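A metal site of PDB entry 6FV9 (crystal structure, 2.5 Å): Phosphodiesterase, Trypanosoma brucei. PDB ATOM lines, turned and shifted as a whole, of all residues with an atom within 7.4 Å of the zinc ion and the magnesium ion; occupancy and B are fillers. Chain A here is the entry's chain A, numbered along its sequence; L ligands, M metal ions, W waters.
The backbone carbonyl oxygen (O) of Ala 148 is in hydrogen-bond range of a ring nitrogen (ND1) of His 151 (2.7 Å).
The nearest printed residue that does not touch the zinc ion is His 111 (4.1 Å).
Of the 21 residues printed, 1 comes within 4 Å of the magnesium ion. The nearest printed residue that does not touch the magnesium ion is Thr 225 (4.05 Å).
The zinc ion is bound by the side-chain carboxylate (OD1) of Asp 264 (2.1 Å), a ring nitrogen (NE2) of His 115 (2.1 Å), the side-chain carboxylate (OD2) of Asp 152 (2.2 Å), water W5 (2.2 Å), water W6 (2.3 Å) and a ring nitrogen (NE2) of His 151 (2.3 Å).
The magnesium ion is bound by water W2 (1.9 Å), water W1 (1.9 Å), water W6 (1.9 Å), water W3 (2.0 Å), the side-chain carboxylate of Asp 152 (2.1 Å) and water W4 (2.3 Å).
Water W3 lies within hydrogen-bond range of OG1 of Thr 225 (2.7 Å) and O of His 151 (2.9 Å). Water W2 lies within hydrogen-bond range of a ring nitrogen (NE2) of His 187 (3.0 Å) and the side-chain carboxylate (OE2) of Glu 184 (3.5 Å). Water W4 lies within hydrogen-bond range of OE2 of Glu 184 (2.7 Å) and O of Thr 225 (2.7 Å).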
ATOM      1  N   TYR A 110      19.197  -8.706 -27.957  1.00  0.00           N
ATOM      2  CA  TYR A 110      17.949  -8.901 -28.707  1.00  0.00           C
ATOM      3  C   TYR A 110      16.934  -7.775 -28.580  1.00  0.00           C
ATOM      4  O   TYR A 110      16.493  -7.250 -29.585  1.00  0.00           O
ATOM      5  CB  TYR A 110      17.314 -10.192 -28.292  1.00  0.00           C
ATOM      6  CG  TYR A 110      16.066 -10.503 -29.061  1.00  0.00           C
ATOM      7  CD1 TYR A 110      16.139 -11.184 -30.252  1.00  0.00           C
ATOM      8  CD2 TYR A 110      14.832 -10.138 -28.582  1.00  0.00           C
ATOM      9  CE1 TYR A 110      14.996 -11.495 -30.953  1.00  0.00           C
ATOM     10  CE2 TYR A 110      13.676 -10.443 -29.282  1.00  0.00           C
ATOM     11  CZ  TYR A 110      13.777 -11.115 -30.462  1.00  0.00           C
ATOM     12  OH  TYR A 110      12.683 -11.472 -31.158  1.00  0.00           O
ATOM     13  N   HIS A 111      16.557  -7.399 -27.360  1.00  0.00           N
ATOM     14  CA  HIS A 111      15.520  -6.361 -27.170  1.00  0.00           C
ATOM     15  C   HIS A 111      16.067  -4.929 -27.241  1.00  0.00           C
ATOM     16  O   HIS A 111      15.938  -4.140 -26.302  1.00  0.00           O
ATOM     17  CB  HIS A 111      14.760  -6.547 -25.869  1.00  0.00           C
ATOM     18  CG  HIS A 111      13.870  -7.736 -25.853  1.00  0.00           C
ATOM     19  ND1 HIS A 111      14.191  -8.913 -25.221  1.00  0.00           N
ATOM     20  CD2 HIS A 111      12.622  -7.910 -26.360  1.00  0.00           C
ATOM     21  CE1 HIS A 111      13.196  -9.773 -25.367  1.00  0.00           C
ATOM     22  NE2 HIS A 111      12.229  -9.189 -26.058  1.00  0.00           N
ATOM     23  N   HIS A 115      15.035  -4.818 -32.816  1.00  0.00           N
ATOM     24  CA  HIS A 115      13.856  -5.684 -32.569  1.00  0.00           C
ATOM     25  C   HIS A 115      12.536  -4.963 -32.862  1.00  0.00           C
ATOM     26  O   HIS A 115      11.661  -5.485 -33.574  1.00  0.00           O
ATOM     27  CB  HIS A 115      13.834  -6.211 -31.146  1.00  0.00           C
ATOM     28  CG  HIS A 115      12.532  -6.835 -30.747  1.00  0.00           C
ATOM     29  ND1 HIS A 115      11.982  -7.903 -31.428  1.00  0.00           N
ATOM     30  CD2 HIS A 115      11.664  -6.531 -29.756  1.00  0.00           C
ATOM     31  CE1 HIS A 115      10.841  -8.240 -30.847  1.00  0.00           C
ATOM     32  NE2 HIS A 115      10.626  -7.423 -29.843  1.00  0.00           N
ATOM     33  N   VAL A 116      12.403  -3.731 -32.368  1.00  0.00           N
ATOM     34  CA  VAL A 116      11.145  -3.009 -32.541  1.00  0.00           C
ATOM     35  C   VAL A 116      10.965  -2.512 -33.973  1.00  0.00           C
ATOM     36  O   VAL A 116       9.827  -2.550 -34.471  1.00  0.00           O
ATOM     37  CB  VAL A 116      10.905  -1.919 -31.465  1.00  0.00           C
ATOM     38  CG1 VAL A 116      11.093  -2.526 -30.082  1.00  0.00           C
ATOM     39  CG2 VAL A 116      11.798  -0.706 -31.630  1.00  0.00           C
ATOM     40  N   VAL A 119       9.757  -5.544 -35.678  1.00  0.00           N
ATOM     41  CA  VAL A 119       8.322  -5.822 -35.398  1.00  0.00           C
ATOM     42  C   VAL A 119       7.452  -4.880 -36.242  1.00  0.00           C
ATOM     43  O   VAL A 119       6.447  -5.313 -36.794  1.00  0.00           O
ATOM     44  CB  VAL A 119       7.994  -5.741 -33.892  1.00  0.00           C
ATOM     45  CG1 VAL A 119       6.490  -5.795 -33.653  1.00  0.00           C
ATOM     46  CG2 VAL A 119       8.663  -6.887 -33.142  1.00  0.00           C
ATOM     47  N   ALA A 148       4.278  -0.842 -32.453  1.00  0.00           N
ATOM     48  CA  ALA A 148       5.464  -1.673 -32.679  1.00  0.00           C
ATOM     49  C   ALA A 148       6.747  -1.008 -32.162  1.00  0.00           C
ATOM     50  O   ALA A 148       7.604  -1.665 -31.586  1.00  0.00           O
ATOM     51  CB  ALA A 148       5.597  -2.009 -34.154  1.00  0.00           C
ATOM     52  N   HIS A 151       6.796  -0.780 -28.070  1.00  0.00           N
ATOM     53  CA  HIS A 151       6.308  -1.932 -27.294  1.00  0.00           C
ATOM     54  C   HIS A 151       7.358  -2.583 -26.349  1.00  0.00           C
ATOM     55  O   HIS A 151       6.984  -3.350 -25.473  1.00  0.00           O
ATOM     56  CB  HIS A 151       5.672  -2.989 -28.224  1.00  0.00           C
ATOM     57  CG  HIS A 151       6.647  -3.989 -28.732  1.00  0.00           C
ATOM     58  ND1 HIS A 151       7.405  -3.776 -29.859  1.00  0.00           N
ATOM     59  CD2 HIS A 151       6.998  -5.215 -28.275  1.00  0.00           C
ATOM     60  CE1 HIS A 151       8.189  -4.819 -30.066  1.00  0.00           C
ATOM     61  NE2 HIS A 151       7.965  -5.709 -29.112  1.00  0.00           N
ATOM     62  N   ASP A 152       8.645  -2.283 -26.525  1.00  0.00           N
ATOM     63  CA  ASP A 152       9.685  -2.755 -25.595  1.00  0.00           C
ATOM     64  C   ASP A 152      10.536  -1.632 -25.024  1.00  0.00           C
ATOM     65  O   ASP A 152      11.664  -1.887 -24.620  1.00  0.00           O
ATOM     66  CB  ASP A 152      10.571  -3.827 -26.268  1.00  0.00           C
ATOM     67  CG  ASP A 152       9.934  -5.244 -26.254  1.00  0.00           C
ATOM     68  OD1 ASP A 152       9.300  -5.676 -25.276  1.00  0.00           O
ATOM     69  OD2 ASP A 152      10.076  -5.949 -27.246  1.00  0.00           O
ATOM     70  N   LEU A 153      10.002  -0.421 -24.978  1.00  0.00           N
ATOM     71  CA  LEU A 153      10.819   0.713 -24.536  1.00  0.00           C
ATOM     72  C   LEU A 153      11.524   0.414 -23.196  1.00  0.00           C
ATOM     73  O   LEU A 153      10.883   0.003 -22.247  1.00  0.00           O
ATOM     74  CB  LEU A 153       9.982   1.993 -24.349  1.00  0.00           C
ATOM     75  CG  LEU A 153       9.476   2.707 -25.577  1.00  0.00           C
ATOM     76  CD1 LEU A 153       8.418   3.704 -25.139  1.00  0.00           C
ATOM     77  CD2 LEU A 153      10.597   3.402 -26.320  1.00  0.00           C
ATOM     78  N   HIS A 155      13.832  -1.862 -22.262  1.00  0.00           N
ATOM     79  CA  HIS A 155      14.035  -3.262 -21.877  1.00  0.00           C
ATOM     80  C   HIS A 155      15.476  -3.412 -21.510  1.00  0.00           C
ATOM     81  O   HIS A 155      16.318  -2.886 -22.202  1.00  0.00           O
ATOM     82  CB  HIS A 155      13.752  -4.166 -23.091  1.00  0.00           C
ATOM     83  CG  HIS A 155      13.302  -5.556 -22.736  1.00  0.00           C
ATOM     84  ND1 HIS A 155      14.162  -6.511 -22.275  1.00  0.00           N
ATOM     85  CD2 HIS A 155      12.089  -6.138 -22.816  1.00  0.00           C
ATOM     86  CE1 HIS A 155      13.501  -7.634 -22.066  1.00  0.00           C
ATOM     87  NE2 HIS A 155      12.242  -7.433 -22.382  1.00  0.00           N
ATOM     88  N   LEU A 183       7.390  -5.374 -17.085  1.00  0.00           N
ATOM     89  CA  LEU A 183       7.960  -4.584 -18.153  1.00  0.00           C
ATOM     90  C   LEU A 183       6.926  -3.979 -19.102  1.00  0.00           C
ATOM     91  O   LEU A 183       7.132  -2.881 -19.577  1.00  0.00           O
ATOM     92  CB  LEU A 183       8.939  -5.406 -18.967  1.00  0.00           C
ATOM     93  CG  LEU A 183      10.178  -5.863 -18.240  1.00  0.00           C
ATOM     94  CD1 LEU A 183      10.795  -6.977 -19.063  1.00  0.00           C
ATOM     95  CD2 LEU A 183      11.160  -4.706 -18.009  1.00  0.00           C
ATOM     96  N   GLU A 184       5.841  -4.701 -19.376  1.00  0.00           N
ATOM     97  CA  GLU A 184       4.788  -4.192 -20.292  1.00  0.00           C
ATOM     98  C   GLU A 184       4.175  -2.900 -19.786  1.00  0.00           C
ATOM     99  O   GLU A 184       3.903  -1.969 -20.579  1.00  0.00           O
ATOM    100  CB  GLU A 184       3.657  -5.207 -20.459  1.00  0.00           C
ATOM    101  CG  GLU A 184       4.006  -6.402 -21.334  1.00  0.00           C
ATOM    102  CD  GLU A 184       4.933  -7.404 -20.677  1.00  0.00           C
ATOM    103  OE1 GLU A 184       5.025  -7.416 -19.425  1.00  0.00           O
ATOM    104  OE2 GLU A 184       5.564  -8.178 -21.422  1.00  0.00           O
ATOM    105  N   HIS A 187       6.838  -0.188 -20.236  1.00  0.00           N
ATOM    106  CA  HIS A 187       6.907   0.268 -21.625  1.00  0.00           C
ATOM    107  C   HIS A 187       5.758   1.251 -21.889  1.00  0.00           C
ATOM    108  O   HIS A 187       5.995   2.295 -22.469  1.00  0.00           O
ATOM    109  CB  HIS A 187       6.826  -0.880 -22.630  1.00  0.00           C
ATOM    110  CG  HIS A 187       7.807  -1.983 -22.424  1.00  0.00           C
ATOM    111  ND1 HIS A 187       9.137  -1.763 -22.114  1.00  0.00           N
ATOM    112  CD2 HIS A 187       7.654  -3.322 -22.521  1.00  0.00           C
ATOM    113  CE1 HIS A 187       9.751  -2.938 -21.999  1.00  0.00           C
ATOM    114  NE2 HIS A 187       8.877  -3.895 -22.244  1.00  0.00           N
ATOM    115  N   VAL A 222       0.245  -3.509 -26.100  1.00  0.00           N
ATOM    116  CA  VAL A 222       1.496  -3.705 -25.381  1.00  0.00           C
ATOM    117  C   VAL A 222       1.324  -4.631 -24.170  1.00  0.00           C
ATOM    118  O   VAL A 222       2.144  -5.496 -23.932  1.00  0.00           O
ATOM    119  CB  VAL A 222       2.148  -2.378 -24.911  1.00  0.00           C
ATOM    120  CG1 VAL A 222       3.424  -2.647 -24.109  1.00  0.00           C
ATOM    121  CG2 VAL A 222       2.480  -1.482 -26.097  1.00  0.00           C
ATOM    122  N   THR A 225       1.393  -8.319 -25.034  1.00  0.00           N
ATOM    123  CA  THR A 225       2.631  -8.990 -25.408  1.00  0.00           C
ATOM    124  C   THR A 225       3.320  -9.739 -24.235  1.00  0.00           C
ATOM    125  O   THR A 225       4.396 -10.326 -24.410  1.00  0.00           O
ATOM    126  CB  THR A 225       3.660  -8.014 -26.086  1.00  0.00           C
ATOM    127  OG1 THR A 225       4.178  -7.075 -25.144  1.00  0.00           O
ATOM    128  CG2 THR A 225       3.027  -7.249 -27.209  1.00  0.00           C
ATOM    129  N   ASP A 226       2.727  -9.706 -23.040  1.00  0.00           N
ATOM    130  CA  ASP A 226       3.201 -10.507 -21.918  1.00  0.00           C
ATOM    131  C   ASP A 226       2.947 -11.964 -22.295  1.00  0.00           C
ATOM    132  O   ASP A 226       1.783 -12.387 -22.412  1.00  0.00           O
ATOM    133  CB  ASP A 226       2.432 -10.106 -20.660  1.00  0.00           C
ATOM    134  CG  ASP A 226       2.906 -10.823 -19.391  1.00  0.00           C
ATOM    135  OD1 ASP A 226       3.696 -11.770 -19.450  1.00  0.00           O
ATOM    136  OD2 ASP A 226       2.466 -10.416 -18.298  1.00  0.00           O
ATOM    137  N   MET A 227       4.018 -12.746 -22.464  1.00  0.00           N
ATOM    138  CA  MET A 227       3.859 -14.141 -22.917  1.00  0.00           C
ATOM    139  C   MET A 227       3.150 -15.073 -21.909  1.00  0.00           C
ATOM    140  O   MET A 227       2.689 -16.135 -22.300  1.00  0.00           O
ATOM    141  CB  MET A 227       5.176 -14.762 -23.409  1.00  0.00           C
ATOM    142  CG  MET A 227       5.574 -14.335 -24.825  1.00  0.00           C
ATOM    143  SD  MET A 227       4.335 -14.531 -26.137  1.00  0.00           S
ATOM    144  CE  MET A 227       4.433 -16.289 -26.493  1.00  0.00           C
ATOM    145  N   LEU A 260       0.193  -7.551 -33.102  1.00  0.00           N
ATOM    146  CA  LEU A 260       1.401  -7.188 -32.357  1.00  0.00           C
ATOM    147  C   LEU A 260       2.074  -8.425 -31.776  1.00  0.00           C
ATOM    148  O   LEU A 260       3.304  -8.588 -31.888  1.00  0.00           O
ATOM    149  CB  LEU A 260       1.138  -6.151 -31.265  1.00  0.00           C
ATOM    150  CG  LEU A 260       2.406  -5.750 -30.459  1.00  0.00           C
ATOM    151  CD1 LEU A 260       3.585  -5.269 -31.320  1.00  0.00           C
ATOM    152  CD2 LEU A 260       2.083  -4.722 -29.397  1.00  0.00           C
ATOM    153  N   GLY A 263       3.898 -10.239 -34.600  1.00  0.00           N
ATOM    154  CA  GLY A 263       5.152  -9.579 -34.876  1.00  0.00           C
ATOM    155  C   GLY A 263       6.199  -9.897 -33.844  1.00  0.00           C
ATOM    156  O   GLY A 263       7.366 -10.054 -34.165  1.00  0.00           O
ATOM    157  N   ASP A 264       5.786  -9.954 -32.588  1.00  0.00           N
ATOM    158  CA  ASP A 264       6.696 -10.252 -31.502  1.00  0.00           C
ATOM    159  C   ASP A 264       7.339 -11.643 -31.595  1.00  0.00           C
ATOM    160  O   ASP A 264       8.500 -11.840 -31.247  1.00  0.00           O
ATOM    161  CB  ASP A 264       5.963 -10.133 -30.157  1.00  0.00           C
ATOM    162  CG  ASP A 264       6.774  -9.419 -29.097  1.00  0.00           C
ATOM    163  OD1 ASP A 264       7.814  -8.839 -29.466  1.00  0.00           O
ATOM    164  OD2 ASP A 264       6.346  -9.399 -27.915  1.00  0.00           O
ATOM    165  N   ILE A 265       6.574 -12.627 -32.065  1.00  0.00           N
ATOM    166  CA  ILE A 265       7.063 -14.000 -32.275  1.00  0.00           C
ATOM    167  C   ILE A 265       7.218 -14.369 -33.772  1.00  0.00           C
ATOM    168  O   ILE A 265       7.073 -15.540 -34.157  1.00  0.00           O
ATOM    169  CB  ILE A 265       6.175 -15.016 -31.542  1.00  0.00           C
ATOM    170  CG1 ILE A 265       4.774 -15.118 -32.152  1.00  0.00           C
ATOM    171  CG2 ILE A 265       6.062 -14.618 -30.083  1.00  0.00           C
ATOM    172  CD1 ILE A 265       4.043 -16.375 -31.792  1.00  0.00           C
HETATM  173  C1  LIG L   1      14.293 -16.215 -32.011  1.00  0.00           C
HETATM  174  C2  LIG L   1      12.995 -16.560 -30.023  1.00  0.00           C
HETATM  175  C3  LIG L   1      12.516 -15.265 -29.970  1.00  0.00           C
HETATM  176  C4  LIG L   1      11.740 -14.838 -28.910  1.00  0.00           C
HETATM  177  C5  LIG L   1      11.430 -15.703 -27.863  1.00  0.00           C
HETATM  178  C6  LIG L   1      11.894 -17.015 -27.906  1.00  0.00           C
HETATM  179  C7  LIG L   1      12.674 -17.451 -28.967  1.00  0.00           C
HETATM  180  C8  LIG L   1      13.232 -19.568 -27.944  1.00  0.00           C
HETATM  181  C9  LIG L   1      10.564 -15.295 -26.723  1.00  0.00           C
HETATM  182  C10 LIG L   1       8.884 -17.020 -24.079  1.00  0.00           C
HETATM  183  C11 LIG L   1       9.992 -17.903 -23.546  1.00  0.00           C
HETATM  184  C12 LIG L   1       9.396 -19.023 -22.725  1.00  0.00           C
HETATM  185  O1  LIG L   1      13.774 -17.088 -31.011  1.00  0.00           O
HETATM  186  O2  LIG L   1      13.186 -18.717 -29.088  1.00  0.00           O
HETATM  187  N1  LIG L   1      10.225 -16.216 -25.890  1.00  0.00           N
HETATM  188  N2  LIG L   1       9.458 -15.871 -24.837  1.00  0.00           N
HETATM  189  N3  LIG L   1       8.482 -19.816 -23.549  1.00  0.00           N
HETATM  190  C13 LIG L   1       7.360 -19.014 -24.069  1.00  0.00           C
HETATM  191  C14 LIG L   1       7.870 -17.830 -24.883  1.00  0.00           C
HETATM  192  C15 LIG L   1       8.744 -21.119 -23.800  1.00  0.00           C
HETATM  193  O3  LIG L   1       9.699 -21.693 -23.279  1.00  0.00           O
HETATM  194  C16 LIG L   1       7.881 -21.867 -24.812  1.00  0.00           C
HETATM  195  N4  LIG L   1       8.461 -23.166 -25.127  1.00  0.00           N
HETATM  196  C17 LIG L   1       9.579 -23.342 -25.921  1.00  0.00           C
HETATM  197  O4  LIG L   1      10.139 -22.453 -26.569  1.00  0.00           O
HETATM  198  C18 LIG L   1       9.995 -24.791 -25.814  1.00  0.00           C
HETATM  199  C19 LIG L   1       8.818 -25.477 -25.171  1.00  0.00           C
HETATM  200  C20 LIG L   1       7.993 -24.363 -24.606  1.00  0.00           C
HETATM  201  O5  LIG L   1       7.085 -24.443 -23.786  1.00  0.00           O
HETATM  202  C21 LIG L   1       9.262 -14.581 -24.408  1.00  0.00           C
HETATM  203  O6  LIG L   1       8.511 -14.337 -23.473  1.00  0.00           O
HETATM  204  C22 LIG L   1       9.996 -13.494 -25.132  1.00  0.00           C
HETATM  205  C23 LIG L   1       9.408 -12.079 -24.958  1.00  0.00           C
HETATM  206  C24 LIG L   1       8.236 -11.830 -25.833  1.00  0.00           C
HETATM  207  C25 LIG L   1       7.913 -12.573 -26.863  1.00  0.00           C
HETATM  208  C26 LIG L   1       8.682 -13.772 -27.293  1.00  0.00           C
HETATM  209  C27 LIG L   1      10.054 -13.889 -26.610  1.00  0.00           C
HETATM  210 ZN    ZN M   1       9.073  -7.570 -28.368  1.00  0.00          ZN
HETATM  211 MG    MG M   2       8.179  -7.368 -24.605  1.00  0.00          MG
HETATM  212  O   HOH W   1       9.686  -8.571 -24.495  1.00  0.00           O
HETATM  213  O   HOH W   2       8.440  -6.810 -22.817  1.00  0.00           O
HETATM  214  O   HOH W   3       6.674  -6.085 -24.649  1.00  0.00           O
HETATM  215  O   HOH W   4       6.550  -8.806 -23.826  1.00  0.00           O
HETATM  216  O   HOH W   5       9.914  -9.489 -27.593  1.00  0.00           O
HETATM  217  O   HOH W   6       7.934  -7.939 -26.434  1.00  0.00           O
